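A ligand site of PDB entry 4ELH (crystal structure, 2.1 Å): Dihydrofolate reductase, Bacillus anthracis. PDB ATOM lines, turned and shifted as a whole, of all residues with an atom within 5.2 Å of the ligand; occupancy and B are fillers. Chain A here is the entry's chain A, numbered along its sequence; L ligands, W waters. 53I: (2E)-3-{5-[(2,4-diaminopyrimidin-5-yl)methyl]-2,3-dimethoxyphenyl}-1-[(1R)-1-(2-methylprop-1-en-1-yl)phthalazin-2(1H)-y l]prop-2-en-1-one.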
ATOM      1  N   MET A   6     -21.730  -6.818   0.459  1.00  0.00           N
ATOM      2  CA  MET A   6     -22.528  -7.764   1.240  1.00  0.00           C
ATOM      3  C   MET A   6     -23.679  -6.986   1.873  1.00  0.00           C
ATOM      4  O   MET A   6     -23.473  -6.008   2.590  1.00  0.00           O
ATOM      5  CB  MET A   6     -21.647  -8.444   2.293  1.00  0.00           C
ATOM      6  CG  MET A   6     -22.388  -9.196   3.380  1.00  0.00           C
ATOM      7  SD  MET A   6     -23.341 -10.574   2.734  1.00  0.00           S
ATOM      8  CE  MET A   6     -22.069 -11.774   2.355  1.00  0.00           C
ATOM      9  N   VAL A   7     -24.910  -7.418   1.584  1.00  0.00           N
ATOM     10  CA  VAL A   7     -26.063  -6.577   1.864  1.00  0.00           C
ATOM     11  C   VAL A   7     -27.335  -7.382   2.175  1.00  0.00           C
ATOM     12  O   VAL A   7     -27.617  -8.414   1.557  1.00  0.00           O
ATOM     13  CB  VAL A   7     -26.328  -5.579   0.698  1.00  0.00           C
ATOM     14  CG1 VAL A   7     -26.505  -6.317  -0.603  1.00  0.00           C
ATOM     15  CG2 VAL A   7     -27.541  -4.718   0.976  1.00  0.00           C
ATOM     16  N   ALA A   8     -28.076  -6.899   3.160  1.00  0.00           N
ATOM     17  CA  ALA A   8     -29.395  -7.454   3.457  1.00  0.00           C
ATOM     18  C   ALA A   8     -30.378  -6.308   3.433  1.00  0.00           C
ATOM     19  O   ALA A   8     -30.213  -5.320   4.152  1.00  0.00           O
ATOM     20  CB  ALA A   8     -29.385  -8.124   4.843  1.00  0.00           C
ATOM     21  N   ILE A  15     -32.054  -0.823   4.552  1.00  0.00           N
ATOM     22  CA  ILE A  15     -30.986  -1.586   5.200  1.00  0.00           C
ATOM     23  C   ILE A  15     -30.801  -1.213   6.675  1.00  0.00           C
ATOM     24  O   ILE A  15     -29.965  -1.797   7.370  1.00  0.00           O
ATOM     25  CB  ILE A  15     -29.634  -1.403   4.489  1.00  0.00           C
ATOM     26  CG1 ILE A  15     -29.214   0.065   4.561  1.00  0.00           C
ATOM     27  CG2 ILE A  15     -29.732  -1.866   3.034  1.00  0.00           C
ATOM     28  CD1 ILE A  15     -27.838   0.362   3.918  1.00  0.00           C
ATOM     29  N   GLY A  16     -31.554  -0.223   7.143  1.00  0.00           N
ATOM     30  CA  GLY A  16     -31.420   0.186   8.542  1.00  0.00           C
ATOM     31  C   GLY A  16     -32.546   1.050   9.074  1.00  0.00           C
ATOM     32  O   GLY A  16     -33.292   1.679   8.313  1.00  0.00           O
ATOM     33  N   ASN A  19     -30.037   3.223  12.900  1.00  0.00           N
ATOM     34  CA  ASN A  19     -28.754   2.512  12.980  1.00  0.00           C
ATOM     35  C   ASN A  19     -28.831   1.027  13.310  1.00  0.00           C
ATOM     36  O   ASN A  19     -27.792   0.403  13.555  1.00  0.00           O
ATOM     37  CB  ASN A  19     -27.799   3.191  13.950  1.00  0.00           C
ATOM     38  CG  ASN A  19     -27.463   4.611  13.530  1.00  0.00           C
ATOM     39  OD1 ASN A  19     -27.308   4.899  12.335  1.00  0.00           O
ATOM     40  ND2 ASN A  19     -27.367   5.502  14.511  1.00  0.00           N
ATOM     41  N   ASN A  20     -30.026   0.444  13.334  1.00  0.00           N
ATOM     42  CA  ASN A  20     -30.097  -1.000  13.526  1.00  0.00           C
ATOM     43  C   ASN A  20     -30.868  -1.745  12.430  1.00  0.00           C
ATOM     44  O   ASN A  20     -31.455  -1.135  11.533  1.00  0.00           O
ATOM     45  CB  ASN A  20     -30.607  -1.330  14.924  1.00  0.00           C
ATOM     46  CG  ASN A  20     -29.663  -0.823  16.002  1.00  0.00           C
ATOM     47  OD1 ASN A  20     -29.800   0.294  16.511  1.00  0.00           O
ATOM     48  ND2 ASN A  20     -28.659  -1.632  16.347  1.00  0.00           N
ATOM     49  N   LEU A  21     -30.812  -3.074  12.480  1.00  0.00           N
ATOM     50  CA  LEU A  21     -31.606  -3.904  11.568  1.00  0.00           C
ATOM     51  C   LEU A  21     -33.052  -3.936  12.035  1.00  0.00           C
ATOM     52  O   LEU A  21     -33.316  -4.220  13.199  1.00  0.00           O
ATOM     53  CB  LEU A  21     -31.077  -5.341  11.524  1.00  0.00           C
ATOM     54  CG  LEU A  21     -29.699  -5.594  10.910  1.00  0.00           C
ATOM     55  CD1 LEU A  21     -29.360  -7.078  10.989  1.00  0.00           C
ATOM     56  CD2 LEU A  21     -29.656  -5.114   9.466  1.00  0.00           C
ATOM     57  N   GLU A  28     -29.735 -15.597   8.724  1.00  0.00           N
ATOM     58  CA  GLU A  28     -29.144 -14.696   7.732  1.00  0.00           C
ATOM     59  C   GLU A  28     -27.727 -14.320   8.138  1.00  0.00           C
ATOM     60  O   GLU A  28     -26.838 -14.318   7.314  1.00  0.00           O
ATOM     61  CB  GLU A  28     -29.996 -13.439   7.513  1.00  0.00           C
ATOM     62  CG  GLU A  28     -29.843 -12.844   6.099  1.00  0.00           C
ATOM     63  CD  GLU A  28     -28.619 -11.923   5.944  1.00  0.00           C
ATOM     64  OE1 GLU A  28     -28.258 -11.231   6.917  1.00  0.00           O
ATOM     65  OE2 GLU A  28     -28.019 -11.880   4.835  1.00  0.00           O
ATOM     66  N   LEU A  29     -27.521 -14.019   9.424  1.00  0.00           N
ATOM     67  CA  LEU A  29     -26.190 -13.646   9.869  1.00  0.00           C
ATOM     68  C   LEU A  29     -25.245 -14.846   9.800  1.00  0.00           C
ATOM     69  O   LEU A  29     -24.067 -14.683   9.546  1.00  0.00           O
ATOM     70  CB  LEU A  29     -26.230 -13.059  11.285  1.00  0.00           C
ATOM     71  CG  LEU A  29     -27.174 -11.855  11.378  1.00  0.00           C
ATOM     72  CD1 LEU A  29     -27.271 -11.297  12.823  1.00  0.00           C
ATOM     73  CD2 LEU A  29     -26.766 -10.755  10.401  1.00  0.00           C
ATOM     74  N   GLN A  30     -25.772 -16.047  10.022  1.00  0.00           N
ATOM     75  CA  GLN A  30     -24.977 -17.260   9.907  1.00  0.00           C
ATOM     76  C   GLN A  30     -24.460 -17.390   8.466  1.00  0.00           C
ATOM     77  O   GLN A  30     -23.350 -17.854   8.218  1.00  0.00           O
ATOM     78  CB  GLN A  30     -25.805 -18.487  10.289  1.00  0.00           C
ATOM     79  CG  GLN A  30     -25.099 -19.467  11.196  1.00  0.00           C
ATOM     80  CD  GLN A  30     -24.196 -18.798  12.216  1.00  0.00           C
ATOM     81  OE1 GLN A  30     -22.998 -19.088  12.272  1.00  0.00           O
ATOM     82  NE2 GLN A  30     -24.759 -17.901  13.016  1.00  0.00           N
ATOM     83  N   VAL A  32     -23.913 -14.764   6.404  1.00  0.00           N
ATOM     84  CA  VAL A  32     -22.885 -13.735   6.324  1.00  0.00           C
ATOM     85  C   VAL A  32     -21.572 -14.263   6.896  1.00  0.00           C
ATOM     86  O   VAL A  32     -20.490 -14.041   6.317  1.00  0.00           O
ATOM     87  CB  VAL A  32     -23.271 -12.483   7.134  1.00  0.00           C
ATOM     88  CG1 VAL A  32     -22.051 -11.555   7.309  1.00  0.00           C
ATOM     89  CG2 VAL A  32     -24.451 -11.760   6.483  1.00  0.00           C
ATOM     90  N   LYS A  33     -21.648 -14.930   8.035  1.00  0.00           N
ATOM     91  CA  LYS A  33     -20.444 -15.406   8.685  1.00  0.00           C
ATOM     92  C   LYS A  33     -19.739 -16.428   7.811  1.00  0.00           C
ATOM     93  O   LYS A  33     -18.534 -16.335   7.574  1.00  0.00           O
ATOM     94  CB  LYS A  33     -20.755 -16.018  10.058  1.00  0.00           C
ATOM     95  CG  LYS A  33     -19.529 -16.531  10.779  1.00  0.00           C
ATOM     96  CD  LYS A  33     -19.887 -17.206  12.098  1.00  0.00           C
ATOM     97  CE  LYS A  33     -18.665 -17.900  12.697  1.00  0.00           C
ATOM     98  NZ  LYS A  33     -18.711 -17.842  14.181  1.00  0.00           N
ATOM     99  N   ASN A  47     -22.087   1.654  11.374  1.00  0.00           N
ATOM    100  CA  ASN A  47     -22.383   0.254  11.205  1.00  0.00           C
ATOM    101  C   ASN A  47     -21.648  -0.545  12.269  1.00  0.00           C
ATOM    102  O   ASN A  47     -22.272  -1.312  13.004  1.00  0.00           O
ATOM    103  CB  ASN A  47     -21.997  -0.205   9.801  1.00  0.00           C
ATOM    104  CG  ASN A  47     -22.988  -1.186   9.210  1.00  0.00           C
ATOM    105  OD1 ASN A  47     -23.998  -0.786   8.637  1.00  0.00           O
ATOM    106  ND2 ASN A  47     -22.714  -2.469   9.354  1.00  0.00           N
ATOM    107  N   ALA A  50     -23.096  -0.125  15.685  1.00  0.00           N
ATOM    108  CA  ALA A  50     -24.408  -0.752  15.810  1.00  0.00           C
ATOM    109  C   ALA A  50     -24.281  -2.236  16.127  1.00  0.00           C
ATOM    110  O   ALA A  50     -25.120  -2.812  16.822  1.00  0.00           O
ATOM    111  CB  ALA A  50     -25.217  -0.552  14.547  1.00  0.00           C
ATOM    112  N   ILE A  51     -23.229  -2.866  15.590  1.00  0.00           N
ATOM    113  CA  ILE A  51     -22.952  -4.268  15.860  1.00  0.00           C
ATOM    114  C   ILE A  51     -22.366  -4.415  17.258  1.00  0.00           C
ATOM    115  O   ILE A  51     -22.617  -5.409  17.940  1.00  0.00           O
ATOM    116  CB  ILE A  51     -21.981  -4.846  14.820  1.00  0.00           C
ATOM    117  CG1 ILE A  51     -22.616  -4.842  13.429  1.00  0.00           C
ATOM    118  CG2 ILE A  51     -21.554  -6.248  15.204  1.00  0.00           C
ATOM    119  CD1 ILE A  51     -21.655  -5.278  12.327  1.00  0.00           C
ATOM    120  N   ARG A  53     -19.304  -4.873  18.479  1.00  0.00           N
ATOM    121  CA  ARG A  53     -18.043  -5.545  18.725  1.00  0.00           C
ATOM    122  C   ARG A  53     -17.442  -6.058  17.426  1.00  0.00           C
ATOM    123  O   ARG A  53     -18.123  -6.102  16.402  1.00  0.00           O
ATOM    124  CB  ARG A  53     -18.249  -6.709  19.681  1.00  0.00           C
ATOM    125  CG  ARG A  53     -19.069  -7.825  19.074  1.00  0.00           C
ATOM    126  CD  ARG A  53     -18.926  -9.093  19.883  1.00  0.00           C
ATOM    127  NE  ARG A  53     -20.165  -9.433  20.573  1.00  0.00           N
ATOM    128  CZ  ARG A  53     -20.689 -10.657  20.591  1.00  0.00           C
ATOM    129  NH1 ARG A  53     -20.071 -11.642  19.957  1.00  0.00           N
ATOM    130  NH2 ARG A  53     -21.827 -10.879  21.240  1.00  0.00           N
ATOM    131  N   PRO A  54     -16.150  -6.436  17.456  1.00  0.00           N
ATOM    132  CA  PRO A  54     -15.511  -7.073  16.293  1.00  0.00           C
ATOM    133  C   PRO A  54     -16.150  -8.430  15.992  1.00  0.00           C
ATOM    134  O   PRO A  54     -16.509  -9.156  16.926  1.00  0.00           O
ATOM    135  CB  PRO A  54     -14.068  -7.277  16.763  1.00  0.00           C
ATOM    136  CG  PRO A  54     -13.874  -6.269  17.833  1.00  0.00           C
ATOM    137  CD  PRO A  54     -15.183  -6.129  18.522  1.00  0.00           C
ATOM    138  N   LEU A  55     -16.283  -8.764  14.718  1.00  0.00           N
ATOM    139  CA  LEU A  55     -16.742 -10.092  14.343  1.00  0.00           C
ATOM    140  C   LEU A  55     -15.523 -10.999  14.163  1.00  0.00           C
ATOM    141  O   LEU A  55     -14.694 -10.765  13.275  1.00  0.00           O
ATOM    142  CB  LEU A  55     -17.599 -10.055  13.078  1.00  0.00           C
ATOM    143  CG  LEU A  55     -18.400  -8.787  12.750  1.00  0.00           C
ATOM    144  CD1 LEU A  55     -19.543  -9.078  11.772  1.00  0.00           C
ATOM    145  CD2 LEU A  55     -18.948  -8.116  13.997  1.00  0.00           C
ATOM    146  N   PRO A  56     -15.402 -12.040  15.001  1.00  0.00           N
ATOM    147  CA  PRO A  56     -14.212 -12.887  15.066  1.00  0.00           C
ATOM    148  C   PRO A  56     -13.957 -13.650  13.774  1.00  0.00           C
ATOM    149  O   PRO A  56     -14.864 -13.774  12.954  1.00  0.00           O
ATOM    150  CB  PRO A  56     -14.558 -13.875  16.188  1.00  0.00           C
ATOM    151  CG  PRO A  56     -16.044 -13.901  16.227  1.00  0.00           C
ATOM    152  CD  PRO A  56     -16.469 -12.503  15.901  1.00  0.00           C
ATOM    153  N   ILE A  95     -17.562  -5.354   1.367  1.00  0.00           N
ATOM    154  CA  ILE A  95     -18.081  -4.065   1.800  1.00  0.00           C
ATOM    155  C   ILE A  95     -19.392  -4.318   2.552  1.00  0.00           C
ATOM    156  O   ILE A  95     -20.364  -4.818   1.978  1.00  0.00           O
ATOM    157  CB  ILE A  95     -18.336  -3.144   0.620  1.00  0.00           C
ATOM    158  CG1 ILE A  95     -17.120  -3.163  -0.313  1.00  0.00           C
ATOM    159  CG2 ILE A  95     -18.671  -1.736   1.101  1.00  0.00           C
ATOM    160  CD1 ILE A  95     -15.818  -2.783   0.385  1.00  0.00           C
ATOM    161  N   PHE A  96     -19.405  -3.959   3.827  1.00  0.00           N
ATOM    162  CA  PHE A  96     -20.437  -4.456   4.721  1.00  0.00           C
ATOM    163  C   PHE A  96     -21.453  -3.392   5.063  1.00  0.00           C
ATOM    164  O   PHE A  96     -22.412  -3.640   5.816  1.00  0.00           O
ATOM    165  CB  PHE A  96     -19.797  -4.981   5.986  1.00  0.00           C
ATOM    166  CG  PHE A  96     -20.675  -5.870   6.776  1.00  0.00           C
ATOM    167  CD1 PHE A  96     -21.179  -7.037   6.218  1.00  0.00           C
ATOM    168  CD2 PHE A  96     -20.974  -5.579   8.092  1.00  0.00           C
ATOM    169  CE1 PHE A  96     -21.981  -7.880   6.958  1.00  0.00           C
ATOM    170  CE2 PHE A  96     -21.774  -6.415   8.840  1.00  0.00           C
ATOM    171  CZ  PHE A  96     -22.278  -7.579   8.265  1.00  0.00           C
ATOM    172  N   GLY A  97     -21.268  -2.209   4.514  1.00  0.00           N
ATOM    173  CA  GLY A  97     -22.332  -1.252   4.577  1.00  0.00           C
ATOM    174  C   GLY A  97     -22.149  -0.069   5.485  1.00  0.00           C
ATOM    175  O   GLY A  97     -21.103   0.139   6.105  1.00  0.00           O
ATOM    176  N   TYR A 102     -21.034   1.877   0.878  1.00  0.00           N
ATOM    177  CA  TYR A 102     -21.328   1.253  -0.416  1.00  0.00           C
ATOM    178  C   TYR A 102     -21.017   2.248  -1.549  1.00  0.00           C
ATOM    179  O   TYR A 102     -20.388   1.899  -2.547  1.00  0.00           O
ATOM    180  CB  TYR A 102     -22.781   0.818  -0.505  1.00  0.00           C
ATOM    181  CG  TYR A 102     -23.164  -0.349   0.389  1.00  0.00           C
ATOM    182  CD1 TYR A 102     -22.374  -1.487   0.470  1.00  0.00           C
ATOM    183  CD2 TYR A 102     -24.309  -0.292   1.184  1.00  0.00           C
ATOM    184  CE1 TYR A 102     -22.728  -2.558   1.295  1.00  0.00           C
ATOM    185  CE2 TYR A 102     -24.684  -1.361   1.996  1.00  0.00           C
ATOM    186  CZ  TYR A 102     -23.890  -2.478   2.057  1.00  0.00           C
ATOM    187  OH  TYR A 102     -24.228  -3.520   2.905  1.00  0.00           O
ATOM    188  N   THR A 115     -29.058 -10.193   0.060  1.00  0.00           N
ATOM    189  CA  THR A 115     -30.170 -10.889   0.687  1.00  0.00           C
ATOM    190  C   THR A 115     -31.380  -9.996   0.542  1.00  0.00           C
ATOM    191  O   THR A 115     -31.340  -8.835   0.961  1.00  0.00           O
ATOM    192  CB  THR A 115     -29.957 -11.169   2.183  1.00  0.00           C
ATOM    193  OG1 THR A 115     -28.789 -11.971   2.380  1.00  0.00           O
ATOM    194  CG2 THR A 115     -31.162 -11.915   2.770  1.00  0.00           C
HETATM  195  O30 53I L   1     -25.160  -8.707  15.632  1.00  0.00           O
HETATM  196  C16 53I L   1     -24.592  -8.670  14.510  1.00  0.00           C
HETATM  197  N17 53I L   1     -23.827  -9.847  14.061  1.00  0.00           N
HETATM  198  N18 53I L   1     -23.204  -9.846  12.846  1.00  0.00           N
HETATM  199  C19 53I L   1     -22.406 -10.959  12.467  1.00  0.00           C
HETATM  200  C25 53I L   1     -22.738 -12.266  13.061  1.00  0.00           C
HETATM  201  C26 53I L   1     -22.383 -13.487  12.397  1.00  0.00           C
HETATM  202  C27 53I L   1     -22.722 -14.734  12.977  1.00  0.00           C
HETATM  203  C28 53I L   1     -23.394 -14.786  14.183  1.00  0.00           C
HETATM  204  C29 53I L   1     -23.737 -13.603  14.823  1.00  0.00           C
HETATM  205  C24 53I L   1     -23.388 -12.312  14.227  1.00  0.00           C
HETATM  206  C20 53I L   1     -23.782 -11.021  14.932  1.00  0.00           C
HETATM  207  C21 53I L   1     -22.911 -10.855  16.170  1.00  0.00           C
HETATM  208  C22 53I L   1     -21.981  -9.871  16.397  1.00  0.00           C
HETATM  209  C23 53I L   1     -22.139  -8.946  17.609  1.00  0.00           C
HETATM  210  C37 53I L   1     -20.540 -10.152  15.960  1.00  0.00           C
HETATM  211  C15 53I L   1     -24.713  -7.393  13.645  1.00  0.00           C
HETATM  212  C14 53I L   1     -24.995  -7.527  12.306  1.00  0.00           C
HETATM  213  C13 53I L   1     -25.455  -6.384  11.475  1.00  0.00           C
HETATM  214  C10 53I L   1     -26.155  -5.277  12.000  1.00  0.00           C
HETATM  215  O11 53I L   1     -26.474  -5.218  13.373  1.00  0.00           O
HETATM  216  C12 53I L   1     -26.378  -4.040  14.084  1.00  0.00           C
HETATM  217  C07 53I L   1     -26.558  -4.254  11.142  1.00  0.00           C
HETATM  218  O08 53I L   1     -27.263  -3.134  11.628  1.00  0.00           O
HETATM  219  C09 53I L   1     -27.675  -2.112  10.717  1.00  0.00           C
HETATM  220  C06 53I L   1     -26.251  -4.329   9.760  1.00  0.00           C
HETATM  221  C05 53I L   1     -25.556  -5.430   9.229  1.00  0.00           C
HETATM  222  C04 53I L   1     -25.239  -5.456   7.756  1.00  0.00           C
HETATM  223  C03 53I L   1     -25.581  -6.706   6.969  1.00  0.00           C
HETATM  224  C32 53I L   1     -26.386  -7.789   7.419  1.00  0.00           C
HETATM  225  N33 53I L   1     -26.598  -8.862   6.554  1.00  0.00           N
HETATM  226  C34 53I L   1     -26.073  -8.870   5.318  1.00  0.00           C
HETATM  227  N35 53I L   1     -26.262  -9.966   4.414  1.00  0.00           N
HETATM  228  N36 53I L   1     -25.290  -7.850   4.891  1.00  0.00           N
HETATM  229  C02 53I L   1     -25.050  -6.772   5.686  1.00  0.00           C
HETATM  230  N01 53I L   1     -24.243  -5.703   5.193  1.00  0.00           N
HETATM  231  C31 53I L   1     -25.153  -6.449  10.071  1.00  0.00           C
HETATM  232  O   HOH W   1     -29.768  -4.616  14.570  1.00  0.00           O
HETATM  233  O   HOH W   2     -27.450  -4.508   4.967  1.00  0.00           O
HETATM  234  O   HOH W   3     -26.546 -15.941  13.738  1.00  0.00           O
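Merely in contact with the ligand: Leu 55 (3.2 Å), Ala 50 (3.3 Å), Val 32 (3.3 Å), Ile 51 (3.3 Å), Leu 21 (3.4 Å), Leu 29 (3.5 Å), Arg 53 (3.6 Å), Gln 30 (3.6 Å), Asn 20 (3.6 Å), Lys 33 (3.7 Å), Asn 19 (3.8 Å) and Thr 115 (3.8 Å). Hydrophobic or aromatic side chains within 4 Å of the ligand: Met 6, Ala 8, Leu 21, Leu 29, Val 32, Ala 50, Ile 51, Leu 55 and Phe 96. Within 4 Å of the ligand: Met 6, Val 7, Ala 8, Asn 19, Asn 20, Leu 21, Glu 28, Leu 29, Gln 30, Val 32, Lys 33, Ala 50, Ile 51, Arg 53, Leu 55, Phe 96, Tyr 102 and Thr 115.
OE2 of Glu 28 is in hydrogen-bond range of OG1 of Thr 115. OH of Tyr 102 lies within hydrogen-bond range of O of Met 6, 2.6 Å away. The backbone carbonyl oxygen of Ile 95 lies within hydrogen-bond range of the backbone NH of Met 6, 2.9 Å away. O of Phe 96 lies within hydrogen-bond range of OH of Tyr 102 (3.4 Å). The backbone carbonyl oxygen of Val 7 is in hydrogen-bond range of the backbone NH of Thr 115, 2.7 Å away.
N35 of the ligand sits at hydrogen-bond distance from OE2 of Glu 28 (2.6 Å). The backbone carbonyl oxygen (O) of Met 6 lies within hydrogen-bond range of a nitrogen (N01) of the ligand (2.7 Å). The side-chain sulfur of Met 6 is in hydrogen-bond range of a nitrogen (N35) of the ligand (3.4 Å). N01 of the ligand is in hydrogen-bond range of O of Phe 96, 2.8 Å away. The side-chain hydroxyl (OH) of Tyr 102 is in hydrogen-bond range of a nitrogen (N01) of the ligand, at 3.2 Å. The backbone NH (N) of Ala 8 lies within hydrogen-bond range of a nitrogen (N36) of the ligand (3.4 Å). The backbone NH of Val 7 is in hydrogen-bond range of a nitrogen (N36) of the ligand (3.4 Å).
Water W2 bridges O of Ala 8 and N01 of the ligand.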
